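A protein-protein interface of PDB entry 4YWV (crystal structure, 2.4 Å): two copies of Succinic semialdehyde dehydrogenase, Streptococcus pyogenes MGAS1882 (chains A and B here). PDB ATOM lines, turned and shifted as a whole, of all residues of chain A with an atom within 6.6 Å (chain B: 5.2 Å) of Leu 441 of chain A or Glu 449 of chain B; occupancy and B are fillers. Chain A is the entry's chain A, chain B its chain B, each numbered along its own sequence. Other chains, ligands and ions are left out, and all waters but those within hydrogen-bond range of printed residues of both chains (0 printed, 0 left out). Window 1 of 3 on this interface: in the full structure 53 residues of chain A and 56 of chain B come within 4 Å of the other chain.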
ATOM      1  N   TYR A  95       8.729  39.808 -25.268  1.00  0.00           N
ATOM      2  CA  TYR A  95       8.926  39.248 -23.945  1.00  0.00           C
ATOM      3  C   TYR A  95       9.552  40.199 -22.928  1.00  0.00           C
ATOM      4  O   TYR A  95       9.277  40.100 -21.724  1.00  0.00           O
ATOM      5  CB  TYR A  95       9.721  37.945 -24.057  1.00  0.00           C
ATOM      6  CG  TYR A  95       8.841  36.834 -24.575  1.00  0.00           C
ATOM      7  CD1 TYR A  95       7.761  36.395 -23.828  1.00  0.00           C
ATOM      8  CD2 TYR A  95       9.030  36.285 -25.838  1.00  0.00           C
ATOM      9  CE1 TYR A  95       6.886  35.446 -24.319  1.00  0.00           C
ATOM     10  CE2 TYR A  95       8.155  35.329 -26.344  1.00  0.00           C
ATOM     11  CZ  TYR A  95       7.081  34.918 -25.575  1.00  0.00           C
ATOM     12  OH  TYR A  95       6.175  34.000 -26.052  1.00  0.00           O
ATOM     13  N   PHE A 102       3.188  38.909 -17.730  1.00  0.00           N
ATOM     14  CA  PHE A 102       3.235  37.448 -17.719  1.00  0.00           C
ATOM     15  C   PHE A 102       3.706  36.777 -16.431  1.00  0.00           C
ATOM     16  O   PHE A 102       3.280  35.664 -16.121  1.00  0.00           O
ATOM     17  CB  PHE A 102       4.086  36.956 -18.896  1.00  0.00           C
ATOM     18  CG  PHE A 102       3.456  37.198 -20.245  1.00  0.00           C
ATOM     19  CD1 PHE A 102       2.236  37.875 -20.355  1.00  0.00           C
ATOM     20  CD2 PHE A 102       4.077  36.746 -21.406  1.00  0.00           C
ATOM     21  CE1 PHE A 102       1.648  38.096 -21.599  1.00  0.00           C
ATOM     22  CE2 PHE A 102       3.497  36.963 -22.662  1.00  0.00           C
ATOM     23  CZ  PHE A 102       2.280  37.641 -22.757  1.00  0.00           C
ATOM     24  N   THR A 409      -5.915  20.165 -36.036  1.00  0.00           N
ATOM     25  CA  THR A 409      -4.584  20.727 -36.180  1.00  0.00           C
ATOM     26  C   THR A 409      -4.415  21.864 -35.174  1.00  0.00           C
ATOM     27  O   THR A 409      -5.399  22.401 -34.648  1.00  0.00           O
ATOM     28  CB  THR A 409      -4.394  21.256 -37.619  1.00  0.00           C
ATOM     29  OG1 THR A 409      -3.038  21.659 -37.815  1.00  0.00           O
ATOM     30  CG2 THR A 409      -5.315  22.441 -37.879  1.00  0.00           C
ATOM     31  N   GLY A 410      -3.169  22.240 -34.916  1.00  0.00           N
ATOM     32  CA  GLY A 410      -2.904  23.298 -33.956  1.00  0.00           C
ATOM     33  C   GLY A 410      -3.131  24.723 -34.419  1.00  0.00           C
ATOM     34  O   GLY A 410      -3.447  25.592 -33.605  1.00  0.00           O
ATOM     35  N   MET A 411      -2.987  24.971 -35.718  1.00  0.00           N
ATOM     36  CA  MET A 411      -3.146  26.320 -36.256  1.00  0.00           C
ATOM     37  C   MET A 411      -3.847  26.374 -37.598  1.00  0.00           C
ATOM     38  O   MET A 411      -3.679  25.491 -38.442  1.00  0.00           O
ATOM     39  CB  MET A 411      -1.775  26.970 -36.405  1.00  0.00           C
ATOM     40  CG  MET A 411      -0.900  26.795 -35.188  1.00  0.00           C
ATOM     41  SD  MET A 411       0.752  27.368 -35.478  1.00  0.00           S
ATOM     42  CE  MET A 411       1.315  26.117 -36.598  1.00  0.00           C
ATOM     43  N   PRO A 425       0.264  31.644 -30.384  1.00  0.00           N
ATOM     44  CA  PRO A 425       0.811  30.353 -29.949  1.00  0.00           C
ATOM     45  C   PRO A 425       1.106  29.449 -31.147  1.00  0.00           C
ATOM     46  O   PRO A 425       0.316  29.365 -32.096  1.00  0.00           O
ATOM     47  CB  PRO A 425      -0.280  29.798 -29.037  1.00  0.00           C
ATOM     48  CG  PRO A 425      -1.522  30.420 -29.582  1.00  0.00           C
ATOM     49  CD  PRO A 425      -1.107  31.834 -29.879  1.00  0.00           C
ATOM     50  N   GLY A 427       2.077  25.550 -32.365  1.00  0.00           N
ATOM     51  CA  GLY A 427       2.118  24.157 -31.969  1.00  0.00           C
ATOM     52  C   GLY A 427       1.103  23.317 -32.709  1.00  0.00           C
ATOM     53  O   GLY A 427       0.257  23.845 -33.428  1.00  0.00           O
ATOM     54  N   ILE A 429      -0.756  18.949 -33.038  1.00  0.00           N
ATOM     55  CA  ILE A 429      -1.184  17.723 -32.373  1.00  0.00           C
ATOM     56  C   ILE A 429      -0.606  16.508 -33.092  1.00  0.00           C
ATOM     57  O   ILE A 429       0.280  16.640 -33.936  1.00  0.00           O
ATOM     58  CB  ILE A 429      -2.718  17.607 -32.332  1.00  0.00           C
ATOM     59  CG1 ILE A 429      -3.284  17.514 -33.751  1.00  0.00           C
ATOM     60  CG2 ILE A 429      -3.322  18.790 -31.589  1.00  0.00           C
ATOM     61  CD1 ILE A 429      -4.793  17.589 -33.812  1.00  0.00           C
ATOM     62  N   GLY A 435       2.292  20.729 -26.772  1.00  0.00           N
ATOM     63  CA  GLY A 435       2.851  21.894 -26.119  1.00  0.00           C
ATOM     64  C   GLY A 435       2.778  23.050 -27.095  1.00  0.00           C
ATOM     65  O   GLY A 435       2.406  22.875 -28.256  1.00  0.00           O
ATOM     66  N   ARG A 436       3.135  24.240 -26.645  1.00  0.00           N
ATOM     67  CA  ARG A 436       3.071  25.394 -27.520  1.00  0.00           C
ATOM     68  C   ARG A 436       4.224  26.325 -27.255  1.00  0.00           C
ATOM     69  O   ARG A 436       4.692  26.437 -26.126  1.00  0.00           O
ATOM     70  CB  ARG A 436       1.761  26.148 -27.295  1.00  0.00           C
ATOM     71  CG  ARG A 436       0.516  25.410 -27.747  1.00  0.00           C
ATOM     72  CD  ARG A 436       0.282  25.614 -29.218  1.00  0.00           C
ATOM     73  NE  ARG A 436      -0.940  24.961 -29.688  1.00  0.00           N
ATOM     74  CZ  ARG A 436      -1.090  23.645 -29.789  1.00  0.00           C
ATOM     75  NH1 ARG A 436      -0.095  22.833 -29.451  1.00  0.00           N
ATOM     76  NH2 ARG A 436      -2.229  23.145 -30.249  1.00  0.00           N
ATOM     77  N   GLU A 437       4.695  26.981 -28.306  1.00  0.00           N
ATOM     78  CA  GLU A 437       5.769  27.942 -28.158  1.00  0.00           C
ATOM     79  C   GLU A 437       5.188  29.283 -28.551  1.00  0.00           C
ATOM     80  O   GLU A 437       4.246  29.349 -29.340  1.00  0.00           O
ATOM     81  CB  GLU A 437       6.957  27.574 -29.042  1.00  0.00           C
ATOM     82  CG  GLU A 437       7.476  26.180 -28.759  1.00  0.00           C
ATOM     83  CD  GLU A 437       8.956  26.013 -29.068  1.00  0.00           C
ATOM     84  OE1 GLU A 437       9.423  26.563 -30.088  1.00  0.00           O
ATOM     85  OE2 GLU A 437       9.653  25.313 -28.295  1.00  0.00           O
ATOM     86  N   LEU A 438       5.736  30.340 -27.963  1.00  0.00           N
ATOM     87  CA  LEU A 438       5.310  31.718 -28.194  1.00  0.00           C
ATOM     88  C   LEU A 438       4.007  32.067 -27.479  1.00  0.00           C
ATOM     89  O   LEU A 438       3.355  31.200 -26.897  1.00  0.00           O
ATOM     90  CB  LEU A 438       5.201  32.013 -29.691  1.00  0.00           C
ATOM     91  CG  LEU A 438       6.541  31.918 -30.414  1.00  0.00           C
ATOM     92  CD1 LEU A 438       6.358  32.264 -31.871  1.00  0.00           C
ATOM     93  CD2 LEU A 438       7.538  32.856 -29.769  1.00  0.00           C
ATOM     94  N   SER A 439       3.648  33.349 -27.528  1.00  0.00           N
ATOM     95  CA  SER A 439       2.464  33.882 -26.857  1.00  0.00           C
ATOM     96  C   SER A 439       2.651  33.579 -25.379  1.00  0.00           C
ATOM     97  O   SER A 439       3.717  33.119 -24.962  1.00  0.00           O
ATOM     98  CB  SER A 439       1.183  33.227 -27.371  1.00  0.00           C
ATOM     99  OG  SER A 439       1.072  31.890 -26.917  1.00  0.00           O
ATOM    100  N   GLU A 440       1.631  33.833 -24.577  1.00  0.00           N
ATOM    101  CA  GLU A 440       1.753  33.566 -23.159  1.00  0.00           C
ATOM    102  C   GLU A 440       1.756  32.061 -22.863  1.00  0.00           C
ATOM    103  O   GLU A 440       2.311  31.624 -21.856  1.00  0.00           O
ATOM    104  CB  GLU A 440       0.629  34.279 -22.405  1.00  0.00           C
ATOM    105  CG  GLU A 440       0.627  34.028 -20.913  1.00  0.00           C
ATOM    106  CD  GLU A 440      -0.032  35.152 -20.127  1.00  0.00           C
ATOM    107  OE1 GLU A 440      -1.076  35.683 -20.579  1.00  0.00           O
ATOM    108  OE2 GLU A 440       0.493  35.496 -19.047  1.00  0.00           O
ATOM    109  N   LEU A 441       1.165  31.265 -23.752  1.00  0.00           N
ATOM    110  CA  LEU A 441       1.116  29.818 -23.557  1.00  0.00           C
ATOM    111  C   LEU A 441       2.496  29.167 -23.537  1.00  0.00           C
ATOM    112  O   LEU A 441       2.752  28.273 -22.735  1.00  0.00           O
ATOM    113  CB  LEU A 441       0.263  29.168 -24.644  1.00  0.00           C
ATOM    114  CG  LEU A 441      -1.139  29.759 -24.792  1.00  0.00           C
ATOM    115  CD1 LEU A 441      -1.948  28.891 -25.739  1.00  0.00           C
ATOM    116  CD2 LEU A 441      -1.823  29.842 -23.435  1.00  0.00           C
ATOM    117  N   GLY A 442       3.384  29.600 -24.423  1.00  0.00           N
ATOM    118  CA  GLY A 442       4.716  29.028 -24.434  1.00  0.00           C
ATOM    119  C   GLY A 442       5.517  29.575 -23.270  1.00  0.00           C
ATOM    120  O   GLY A 442       6.453  28.943 -22.767  1.00  0.00           O
ATOM    121  N   PHE A 443       5.129  30.765 -22.830  1.00  0.00           N
ATOM    122  CA  PHE A 443       5.802  31.424 -21.724  1.00  0.00           C
ATOM    123  C   PHE A 443       5.805  30.581 -20.469  1.00  0.00           C
ATOM    124  O   PHE A 443       6.780  30.591 -19.726  1.00  0.00           O
ATOM    125  CB  PHE A 443       5.133  32.752 -21.407  1.00  0.00           C
ATOM    126  CG  PHE A 443       5.810  33.512 -20.315  1.00  0.00           C
ATOM    127  CD1 PHE A 443       7.008  34.180 -20.557  1.00  0.00           C
ATOM    128  CD2 PHE A 443       5.256  33.561 -19.040  1.00  0.00           C
ATOM    129  CE1 PHE A 443       7.648  34.892 -19.545  1.00  0.00           C
ATOM    130  CE2 PHE A 443       5.886  34.268 -18.017  1.00  0.00           C
ATOM    131  CZ  PHE A 443       7.085  34.937 -18.272  1.00  0.00           C
ATOM    132  N   THR A 444       4.721  29.848 -20.231  1.00  0.00           N
ATOM    133  CA  THR A 444       4.617  29.020 -19.024  1.00  0.00           C
ATOM    134  C   THR A 444       4.958  27.537 -19.149  1.00  0.00           C
ATOM    135  O   THR A 444       4.774  26.795 -18.195  1.00  0.00           O
ATOM    136  CB  THR A 444       3.198  29.100 -18.397  1.00  0.00           C
ATOM    137  OG1 THR A 444       2.219  28.765 -19.386  1.00  0.00           O
ATOM    138  CG2 THR A 444       2.920  30.490 -17.851  1.00  0.00           C
ATOM    139  N   SER A 445       5.453  27.096 -20.299  1.00  0.00           N
ATOM    140  CA  SER A 445       5.785  25.676 -20.464  1.00  0.00           C
ATOM    141  C   SER A 445       6.681  25.100 -19.366  1.00  0.00           C
ATOM    142  O   SER A 445       6.538  23.935 -18.982  1.00  0.00           O
ATOM    143  CB  SER A 445       6.448  25.436 -21.826  1.00  0.00           C
ATOM    144  OG  SER A 445       5.550  25.729 -22.882  1.00  0.00           O
ATOM    145  N   TYR B 117      -8.086  31.493 -30.107  1.00  0.00           N
ATOM    146  CA  TYR B 117      -7.836  30.074 -30.180  1.00  0.00           C
ATOM    147  C   TYR B 117      -8.957  29.351 -29.479  1.00  0.00           C
ATOM    148  O   TYR B 117      -9.420  29.780 -28.427  1.00  0.00           O
ATOM    149  CB  TYR B 117      -6.462  29.718 -29.590  1.00  0.00           C
ATOM    150  CG  TYR B 117      -6.293  29.911 -28.099  1.00  0.00           C
ATOM    151  CD1 TYR B 117      -6.804  28.984 -27.186  1.00  0.00           C
ATOM    152  CD2 TYR B 117      -5.571  30.998 -27.601  1.00  0.00           C
ATOM    153  CE1 TYR B 117      -6.593  29.129 -25.814  1.00  0.00           C
ATOM    154  CE2 TYR B 117      -5.356  31.155 -26.235  1.00  0.00           C
ATOM    155  CZ  TYR B 117      -5.867  30.218 -25.346  1.00  0.00           C
ATOM    156  OH  TYR B 117      -5.646  30.380 -23.994  1.00  0.00           O
ATOM    157  N   LEU B 118      -9.413  28.270 -30.103  1.00  0.00           N
ATOM    158  CA  LEU B 118     -10.492  27.457 -29.563  1.00  0.00           C
ATOM    159  C   LEU B 118      -9.894  26.438 -28.610  1.00  0.00           C
ATOM    160  O   LEU B 118      -8.683  26.215 -28.615  1.00  0.00           O
ATOM    161  CB  LEU B 118     -11.214  26.721 -30.692  1.00  0.00           C
ATOM    162  CG  LEU B 118     -11.834  27.540 -31.826  1.00  0.00           C
ATOM    163  CD1 LEU B 118     -12.153  26.622 -32.984  1.00  0.00           C
ATOM    164  CD2 LEU B 118     -13.082  28.258 -31.340  1.00  0.00           C
ATOM    165  N   LYS B 119     -10.743  25.838 -27.782  1.00  0.00           N
ATOM    166  CA  LYS B 119     -10.304  24.813 -26.843  1.00  0.00           C
ATOM    167  C   LYS B 119     -11.027  23.534 -27.240  1.00  0.00           C
ATOM    168  O   LYS B 119     -12.181  23.330 -26.900  1.00  0.00           O
ATOM    169  CB  LYS B 119     -10.641  25.222 -25.406  1.00  0.00           C
ATOM    170  CG  LYS B 119      -9.954  26.516 -25.001  1.00  0.00           C
ATOM    171  CD  LYS B 119      -9.614  26.557 -23.523  1.00  0.00           C
ATOM    172  CE  LYS B 119      -8.846  27.823 -23.180  1.00  0.00           C
ATOM    173  NZ  LYS B 119      -8.353  27.828 -21.773  1.00  0.00           N
ATOM    174  N   THR B 444      -6.911  22.101 -19.113  1.00  0.00           N
ATOM    175  CA  THR B 444      -6.335  22.189 -20.452  1.00  0.00           C
ATOM    176  C   THR B 444      -5.172  21.250 -20.762  1.00  0.00           C
ATOM    177  O   THR B 444      -4.624  21.301 -21.861  1.00  0.00           O
ATOM    178  CB  THR B 444      -5.851  23.604 -20.748  1.00  0.00           C
ATOM    179  OG1 THR B 444      -4.852  23.967 -19.791  1.00  0.00           O
ATOM    180  CG2 THR B 444      -6.999  24.594 -20.666  1.00  0.00           C
ATOM    181  N   VAL B 447      -5.964  19.472 -23.898  1.00  0.00           N
ATOM    182  CA  VAL B 447      -6.828  20.264 -24.746  1.00  0.00           C
ATOM    183  C   VAL B 447      -5.952  20.712 -25.893  1.00  0.00           C
ATOM    184  O   VAL B 447      -4.754  20.940 -25.712  1.00  0.00           O
ATOM    185  CB  VAL B 447      -7.341  21.521 -24.010  1.00  0.00           C
ATOM    186  CG1 VAL B 447      -7.708  22.604 -25.007  1.00  0.00           C
ATOM    187  CG2 VAL B 447      -8.543  21.168 -23.164  1.00  0.00           C
ATOM    188  N   ASN B 448      -6.527  20.805 -27.083  1.00  0.00           N
ATOM    189  CA  ASN B 448      -5.756  21.290 -28.211  1.00  0.00           C
ATOM    190  C   ASN B 448      -6.120  22.759 -28.374  1.00  0.00           C
ATOM    191  O   ASN B 448      -7.257  23.095 -28.695  1.00  0.00           O
ATOM    192  CB  ASN B 448      -6.084  20.502 -29.487  1.00  0.00           C
ATOM    193  CG  ASN B 448      -5.739  21.269 -30.769  1.00  0.00           C
ATOM    194  OD1 ASN B 448      -4.808  22.076 -30.804  1.00  0.00           O
ATOM    195  ND2 ASN B 448      -6.488  21.004 -31.830  1.00  0.00           N
ATOM    196  N   GLU B 449      -5.175  23.644 -28.098  1.00  0.00           N
ATOM    197  CA  GLU B 449      -5.462  25.054 -28.275  1.00  0.00           C
ATOM    198  C   GLU B 449      -5.250  25.297 -29.762  1.00  0.00           C
ATOM    199  O   GLU B 449      -4.123  25.380 -30.256  1.00  0.00           O
ATOM    200  CB  GLU B 449      -4.536  25.899 -27.411  1.00  0.00           C
ATOM    201  CG  GLU B 449      -4.797  25.686 -25.938  1.00  0.00           C
ATOM    202  CD  GLU B 449      -3.543  25.306 -25.183  1.00  0.00           C
ATOM    203  OE1 GLU B 449      -2.794  24.424 -25.677  1.00  0.00           O
ATOM    204  OE2 GLU B 449      -3.312  25.882 -24.093  1.00  0.00           O
ATOM    205  N   HIS B 450      -6.368  25.374 -30.469  1.00  0.00           N
ATOM    206  CA  HIS B 450      -6.385  25.541 -31.908  1.00  0.00           C
ATOM    207  C   HIS B 450      -6.453  27.010 -32.280  1.00  0.00           C
ATOM    208  O   HIS B 450      -7.451  27.677 -32.025  1.00  0.00           O
ATOM    209  CB  HIS B 450      -7.585  24.752 -32.454  1.00  0.00           C
ATOM    210  CG  HIS B 450      -7.675  24.699 -33.946  1.00  0.00           C
ATOM    211  ND1 HIS B 450      -8.497  23.808 -34.601  1.00  0.00           N
ATOM    212  CD2 HIS B 450      -7.086  25.449 -34.909  1.00  0.00           C
ATOM    213  CE1 HIS B 450      -8.411  24.011 -35.904  1.00  0.00           C
ATOM    214  NE2 HIS B 450      -7.564  25.002 -36.118  1.00  0.00           N
ATOM    215  N   LEU B 451      -5.384  27.508 -32.888  1.00  0.00           N
ATOM    216  CA  LEU B 451      -5.326  28.907 -33.287  1.00  0.00           C
ATOM    217  C   LEU B 451      -5.967  29.175 -34.636  1.00  0.00           C
ATOM    218  O   LEU B 451      -5.788  28.417 -35.585  1.00  0.00           O
ATOM    219  CB  LEU B 451      -3.876  29.396 -33.343  1.00  0.00           C
ATOM    220  CG  LEU B 451      -3.650  30.782 -33.964  1.00  0.00           C
ATOM    221  CD1 LEU B 451      -4.023  31.863 -32.972  1.00  0.00           C
ATOM    222  CD2 LEU B 451      -2.198  30.944 -34.357  1.00  0.00           C
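OG of Ser 445 of chain A sits at hydrogen-bond distance from O of Arg 436 of chain A (3.4 Å).
OG of Ser 439 of chain A lies close to N of Leu 441 of chain A (3.2 Å).
The side-chain hydroxyl of Thr 444 of chain A sits at hydrogen-bond distance from the backbone carbonyl oxygen of Leu 441 of chain A (3.4 Å).
The backbone carbonyl oxygen (O) of His 450 of chain B sits at hydrogen-bond distance from the backbone NH (N) of Leu 118 of chain B (2.8 Å).
Position printed for both chains: 444.
Among the printed residues, pairs that only touch across the chains: Gly 410 of chain A with Asn 448 of chain B (3.9 Å), Gly 410 of chain A with His 450 of chain B (3.4 Å), Met 411 of chain A with Leu 451 of chain B (3.4 Å), Pro 425 of chain A with Leu 451 of chain B (3.7 Å), Ile 429 of chain A with Asn 448 of chain B (3.6 Å), Leu 441 of chain A with Tyr 117 of chain B (3.9 Å) and Leu 441 of chain A with Glu 449 of chain B (3.7 Å).
Gly 427 of chain A touches none of the printed residues of chain B.
Of the printed residues of chain B, Ile 429 of chain A touches Asn 448 (3.6 Å).
Of the printed residues of chain B, Arg 436 of chain A touches Asn 448 and Glu 449.
Leu 438 of chain A touches none of the printed residues of chain B.
Of the printed residues of chain B, Leu 441 of chain A touches Tyr 117 (3.9 Å) and Glu 449 (3.7 Å).
Printed residues of chain A within 4 Å of Tyr 117 of chain B: Leu 441 (3.9 Å).
Glu 449 of chain B touches three residues of chain A.
Of the printed residues of chain A, His 450 of chain B touches Thr 409 and Gly 410.
Of the printed residues of chain A, Leu 451 of chain B touches Gly 410 (2.8 Å), Met 411 (3.4 Å) and Pro 425 (3.7 Å).
Hydrophobic or aromatic side chains of chain A that line the printed part of chain B: Ile 429 and Leu 441.
Of the 9 printed residues of chain B, 5 touch a printed residue of chain A.
Hydrophobic or aromatic side chains of chain B that line the printed part of chain A: Tyr 117, His 450 and Leu 451.
The backbone carbonyl oxygen (O) of Thr 409 of chain A lies within hydrogen-bond range of the side-chain amide nitrogen (ND2) of Asn 448 of chain B (3.3 Å).
O of Thr 409 of chain A lies close to ND1 of His 450 of chain B, at 3.4 Å.
O of Gly 410 of chain A is in hydrogen-bond range of N of Leu 451 of chain B, at 2.8 Å.
OD1 of Asn 448 of chain B lies within hydrogen-bond range of NH2 of Arg 436 of chain A, at 2.8 Å.
The backbone carbonyl oxygen (O) of Glu 449 of chain B lies within hydrogen-bond range of the guanidinium group (NH2) of Arg 436 of chain A, 2.9 Å away.
The backbone carbonyl oxygen of Gly 410 of chain A lies close to the backbone carbonyl oxygen of Glu 449 of chain B, at 3.4 Å.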
